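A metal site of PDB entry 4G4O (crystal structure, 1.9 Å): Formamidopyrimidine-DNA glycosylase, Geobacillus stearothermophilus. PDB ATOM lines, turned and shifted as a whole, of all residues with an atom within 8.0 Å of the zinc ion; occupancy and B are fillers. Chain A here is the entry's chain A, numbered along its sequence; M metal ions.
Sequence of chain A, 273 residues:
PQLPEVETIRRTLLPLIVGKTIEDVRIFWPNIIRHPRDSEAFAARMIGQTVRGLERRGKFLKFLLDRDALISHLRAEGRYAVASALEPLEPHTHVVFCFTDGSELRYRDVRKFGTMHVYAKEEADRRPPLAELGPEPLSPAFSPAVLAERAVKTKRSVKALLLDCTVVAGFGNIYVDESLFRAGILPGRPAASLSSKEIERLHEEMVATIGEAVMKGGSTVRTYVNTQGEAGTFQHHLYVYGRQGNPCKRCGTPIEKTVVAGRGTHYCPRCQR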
ATOM      1  N   PHE A 181     -11.636  18.429  17.362  1.00  0.00           N
ATOM      2  CA  PHE A 181     -10.611  18.525  16.316  1.00  0.00           C
ATOM      3  C   PHE A 181     -10.138  17.155  15.832  1.00  0.00           C
ATOM      4  O   PHE A 181     -10.082  16.879  14.628  1.00  0.00           O
ATOM      5  CB  PHE A 181      -9.376  19.297  16.792  1.00  0.00           C
ATOM      6  CG  PHE A 181      -8.241  19.192  15.828  1.00  0.00           C
ATOM      7  CD1 PHE A 181      -8.200  20.009  14.707  1.00  0.00           C
ATOM      8  CD2 PHE A 181      -7.254  18.226  16.002  1.00  0.00           C
ATOM      9  CE1 PHE A 181      -7.165  19.907  13.789  1.00  0.00           C
ATOM     10  CE2 PHE A 181      -6.229  18.111  15.080  1.00  0.00           C
ATOM     11  CZ  PHE A 181      -6.182  18.946  13.984  1.00  0.00           C
ATOM     12  N   TYR A 239      -3.622  20.398  19.887  1.00  0.00           N
ATOM     13  CA  TYR A 239      -3.802  20.665  18.464  1.00  0.00           C
ATOM     14  C   TYR A 239      -4.428  22.025  18.221  1.00  0.00           C
ATOM     15  O   TYR A 239      -4.084  22.702  17.256  1.00  0.00           O
ATOM     16  CB  TYR A 239      -4.665  19.595  17.816  1.00  0.00           C
ATOM     17  CG  TYR A 239      -3.969  18.287  17.607  1.00  0.00           C
ATOM     18  CD1 TYR A 239      -4.182  17.220  18.473  1.00  0.00           C
ATOM     19  CD2 TYR A 239      -3.099  18.104  16.531  1.00  0.00           C
ATOM     20  CE1 TYR A 239      -3.545  16.005  18.269  1.00  0.00           C
ATOM     21  CE2 TYR A 239      -2.463  16.888  16.328  1.00  0.00           C
ATOM     22  CZ  TYR A 239      -2.688  15.849  17.208  1.00  0.00           C
ATOM     23  OH  TYR A 239      -2.053  14.640  17.012  1.00  0.00           O
ATOM     24  N   VAL A 240      -5.369  22.417  19.071  1.00  0.00           N
ATOM     25  CA  VAL A 240      -6.116  23.638  18.804  1.00  0.00           C
ATOM     26  C   VAL A 240      -6.284  24.563  20.000  1.00  0.00           C
ATOM     27  O   VAL A 240      -6.277  25.781  19.840  1.00  0.00           O
ATOM     28  CB  VAL A 240      -7.516  23.343  18.205  1.00  0.00           C
ATOM     29  CG1 VAL A 240      -7.386  22.596  16.867  1.00  0.00           C
ATOM     30  CG2 VAL A 240      -8.388  22.554  19.198  1.00  0.00           C
ATOM     31  N   PRO A 247      -0.517  27.775  13.012  1.00  0.00           N
ATOM     32  CA  PRO A 247      -0.848  26.758  12.003  1.00  0.00           C
ATOM     33  C   PRO A 247      -1.359  25.461  12.642  1.00  0.00           C
ATOM     34  O   PRO A 247      -0.814  24.972  13.629  1.00  0.00           O
ATOM     35  CB  PRO A 247       0.489  26.504  11.289  1.00  0.00           C
ATOM     36  CG  PRO A 247       1.338  27.701  11.608  1.00  0.00           C
ATOM     37  CD  PRO A 247       0.916  28.119  12.985  1.00  0.00           C
ATOM     38  N   CYS A 248      -2.421  24.913  12.048  1.00  0.00           N
ATOM     39  CA  CYS A 248      -2.869  23.580  12.413  1.00  0.00           C
ATOM     40  C   CYS A 248      -1.695  22.617  12.262  1.00  0.00           C
ATOM     41  O   CYS A 248      -0.933  22.721  11.309  1.00  0.00           O
ATOM     42  CB  CYS A 248      -4.006  23.137  11.496  1.00  0.00           C
ATOM     43  SG  CYS A 248      -4.523  21.435  11.789  1.00  0.00           S
ATOM     44  N   LYS A 249      -1.579  21.677  13.185  1.00  0.00           N
ATOM     45  CA  LYS A 249      -0.472  20.715  13.166  1.00  0.00           C
ATOM     46  C   LYS A 249      -0.669  19.606  12.139  1.00  0.00           C
ATOM     47  O   LYS A 249       0.289  18.916  11.777  1.00  0.00           O
ATOM     48  CB  LYS A 249      -0.237  20.129  14.575  1.00  0.00           C
ATOM     49  CG  LYS A 249       0.270  21.160  15.575  1.00  0.00           C
ATOM     50  CD  LYS A 249       0.553  20.529  16.939  1.00  0.00           C
ATOM     51  CE  LYS A 249       1.094  21.575  17.919  1.00  0.00           C
ATOM     52  NZ  LYS A 249       1.360  21.022  19.280  1.00  0.00           N
ATOM     53  N   ARG A 250      -1.905  19.439  11.658  1.00  0.00           N
ATOM     54  CA  ARG A 250      -2.204  18.436  10.643  1.00  0.00           C
ATOM     55  C   ARG A 250      -2.232  18.994   9.215  1.00  0.00           C
ATOM     56  O   ARG A 250      -1.821  18.318   8.273  1.00  0.00           O
ATOM     57  CB  ARG A 250      -3.541  17.749  10.959  1.00  0.00           C
ATOM     58  CG  ARG A 250      -3.526  16.969  12.268  1.00  0.00           C
ATOM     59  CD  ARG A 250      -3.415  15.477  12.048  1.00  0.00           C
ATOM     60  NE  ARG A 250      -3.420  14.724  13.305  1.00  0.00           N
ATOM     61  CZ  ARG A 250      -4.534  14.316  13.926  1.00  0.00           C
ATOM     62  NH1 ARG A 250      -5.730  14.600  13.417  1.00  0.00           N
ATOM     63  NH2 ARG A 250      -4.431  13.639  15.060  1.00  0.00           N
ATOM     64  N   CYS A 251      -2.710  20.218   9.031  1.00  0.00           N
ATOM     65  CA  CYS A 251      -2.864  20.721   7.666  1.00  0.00           C
ATOM     66  C   CYS A 251      -2.268  22.096   7.437  1.00  0.00           C
ATOM     67  O   CYS A 251      -2.254  22.581   6.300  1.00  0.00           O
ATOM     68  CB  CYS A 251      -4.349  20.752   7.292  1.00  0.00           C
ATOM     69  SG  CYS A 251      -5.230  22.111   8.135  1.00  0.00           S
ATOM     70  N   GLY A 252      -1.817  22.751   8.505  1.00  0.00           N
ATOM     71  CA  GLY A 252      -1.171  24.052   8.373  1.00  0.00           C
ATOM     72  C   GLY A 252      -2.109  25.255   8.297  1.00  0.00           C
ATOM     73  O   GLY A 252      -1.663  26.399   8.327  1.00  0.00           O
ATOM     74  N   THR A 253      -3.406  24.992   8.215  1.00  0.00           N
ATOM     75  CA  THR A 253      -4.407  26.073   8.230  1.00  0.00           C
ATOM     76  C   THR A 253      -4.432  26.787   9.601  1.00  0.00           C
ATOM     77  O   THR A 253      -4.390  26.135  10.638  1.00  0.00           O
ATOM     78  CB  THR A 253      -5.798  25.508   7.910  1.00  0.00           C
ATOM     79  OG1 THR A 253      -5.770  24.856   6.634  1.00  0.00           O
ATOM     80  CG2 THR A 253      -6.852  26.622   7.890  1.00  0.00           C
ATOM     81  N   PRO A 254      -4.483  28.131   9.601  1.00  0.00           N
ATOM     82  CA  PRO A 254      -4.486  28.816  10.908  1.00  0.00           C
ATOM     83  C   PRO A 254      -5.652  28.411  11.793  1.00  0.00           C
ATOM     84  O   PRO A 254      -6.800  28.423  11.362  1.00  0.00           O
ATOM     85  CB  PRO A 254      -4.583  30.298  10.536  1.00  0.00           C
ATOM     86  CG  PRO A 254      -3.950  30.361   9.147  1.00  0.00           C
ATOM     87  CD  PRO A 254      -4.365  29.069   8.472  1.00  0.00           C
ATOM     88  N   ILE A 255      -5.357  28.040  13.033  1.00  0.00           N
ATOM     89  CA  ILE A 255      -6.393  27.746  14.006  1.00  0.00           C
ATOM     90  C   ILE A 255      -7.215  28.998  14.278  1.00  0.00           C
ATOM     91  O   ILE A 255      -6.680  30.093  14.363  1.00  0.00           O
ATOM     92  CB  ILE A 255      -5.793  27.215  15.327  1.00  0.00           C
ATOM     93  CG1 ILE A 255      -5.042  25.900  15.042  1.00  0.00           C
ATOM     94  CG2 ILE A 255      -6.892  26.999  16.368  1.00  0.00           C
ATOM     95  CD1 ILE A 255      -5.861  24.901  14.184  1.00  0.00           C
ATOM     96  N   TYR A 267     -10.615  25.831  16.818  1.00  0.00           N
ATOM     97  CA  TYR A 267     -10.845  24.784  15.812  1.00  0.00           C
ATOM     98  C   TYR A 267     -10.065  25.062  14.533  1.00  0.00           C
ATOM     99  O   TYR A 267      -9.635  26.192  14.282  1.00  0.00           O
ATOM    100  CB  TYR A 267     -12.335  24.675  15.489  1.00  0.00           C
ATOM    101  CG  TYR A 267     -12.917  25.954  14.913  1.00  0.00           C
ATOM    102  CD1 TYR A 267     -12.965  26.166  13.533  1.00  0.00           C
ATOM    103  CD2 TYR A 267     -13.388  26.969  15.745  1.00  0.00           C
ATOM    104  CE1 TYR A 267     -13.468  27.340  13.006  1.00  0.00           C
ATOM    105  CE2 TYR A 267     -13.902  28.164  15.225  1.00  0.00           C
ATOM    106  CZ  TYR A 267     -13.942  28.325  13.849  1.00  0.00           C
ATOM    107  OH  TYR A 267     -14.443  29.487  13.307  1.00  0.00           O
ATOM    108  N   CYS A 268      -9.878  24.004  13.740  1.00  0.00           N
ATOM    109  CA  CYS A 268      -9.315  24.148  12.404  1.00  0.00           C
ATOM    110  C   CYS A 268     -10.445  24.076  11.402  1.00  0.00           C
ATOM    111  O   CYS A 268     -11.156  23.059  11.340  1.00  0.00           O
ATOM    112  CB  CYS A 268      -8.311  23.038  12.110  1.00  0.00           C
ATOM    113  SG  CYS A 268      -7.734  23.101  10.384  1.00  0.00           S
ATOM    114  N   PRO A 269     -10.647  25.145  10.620  1.00  0.00           N
ATOM    115  CA  PRO A 269     -11.777  25.166   9.686  1.00  0.00           C
ATOM    116  C   PRO A 269     -11.573  24.264   8.464  1.00  0.00           C
ATOM    117  O   PRO A 269     -12.496  24.103   7.690  1.00  0.00           O
ATOM    118  CB  PRO A 269     -11.843  26.638   9.262  1.00  0.00           C
ATOM    119  CG  PRO A 269     -10.437  27.109   9.387  1.00  0.00           C
ATOM    120  CD  PRO A 269      -9.869  26.399  10.589  1.00  0.00           C
ATOM    121  N   ARG A 270     -10.385  23.673   8.295  1.00  0.00           N
ATOM    122  CA  ARG A 270     -10.193  22.678   7.227  1.00  0.00           C
ATOM    123  C   ARG A 270     -10.323  21.229   7.716  1.00  0.00           C
ATOM    124  O   ARG A 270     -10.995  20.426   7.074  1.00  0.00           O
ATOM    125  CB  ARG A 270      -8.842  22.854   6.551  1.00  0.00           C
ATOM    126  CG  ARG A 270      -8.517  21.729   5.562  1.00  0.00           C
ATOM    127  CD  ARG A 270      -7.199  22.012   4.818  1.00  0.00           C
ATOM    128  NE  ARG A 270      -7.006  21.038   3.746  1.00  0.00           N
ATOM    129  CZ  ARG A 270      -5.967  21.006   2.914  1.00  0.00           C
ATOM    130  NH1 ARG A 270      -5.920  20.071   1.968  1.00  0.00           N
ATOM    131  NH2 ARG A 270      -4.973  21.894   3.028  1.00  0.00           N
ATOM    132  N   CYS A 271      -9.664  20.890   8.821  1.00  0.00           N
ATOM    133  CA  CYS A 271      -9.770  19.543   9.362  1.00  0.00           C
ATOM    134  C   CYS A 271     -11.161  19.231   9.907  1.00  0.00           C
ATOM    135  O   CYS A 271     -11.577  18.079   9.876  1.00  0.00           O
ATOM    136  CB  CYS A 271      -8.730  19.286  10.464  1.00  0.00           C
ATOM    137  SG  CYS A 271      -7.020  19.253   9.854  1.00  0.00           S
ATOM    138  N   GLN A 272     -11.865  20.230  10.424  1.00  0.00           N
ATOM    139  CA  GLN A 272     -13.161  19.986  11.060  1.00  0.00           C
ATOM    140  C   GLN A 272     -14.297  20.443  10.168  1.00  0.00           C
ATOM    141  O   GLN A 272     -14.233  21.524   9.593  1.00  0.00           O
ATOM    142  CB  GLN A 272     -13.241  20.717  12.406  1.00  0.00           C
ATOM    143  CG  GLN A 272     -12.254  20.150  13.417  1.00  0.00           C
ATOM    144  CD  GLN A 272     -12.085  21.018  14.653  1.00  0.00           C
ATOM    145  OE1 GLN A 272     -11.052  21.658  14.837  1.00  0.00           O
ATOM    146  NE2 GLN A 272     -13.086  20.995  15.537  1.00  0.00           N
HETATM  147 ZN    ZN M   1      -6.177  21.410  10.093  1.00  0.00          ZN
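The zinc ion is bound by SG of Cys 251, SG of Cys 268, SG of Cys 271 and SG of Cys 248.
The zinc ion has four donor atoms within binding distance.
Of the 18 residues printed, 4 come within 4 Å of the zinc ion.
The side-chain hydroxyl (OG1) of Thr 253 sits close to the side-chain sulfur (SG) of Cys 251 (3.2 Å).
The side-chain sulfur (SG) of Cys 268 sits close to the backbone NH (N) of Arg 270 (3.4 Å).
The side-chain amide oxygen of Gln 272 lies within hydrogen-bond range of the backbone NH of Cys 268 (2.8 Å).
N of Arg 250 sits close to SG of Cys 248.
N of Cys 248 sits at hydrogen-bond distance from O of Thr 253 (2.7 Å).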
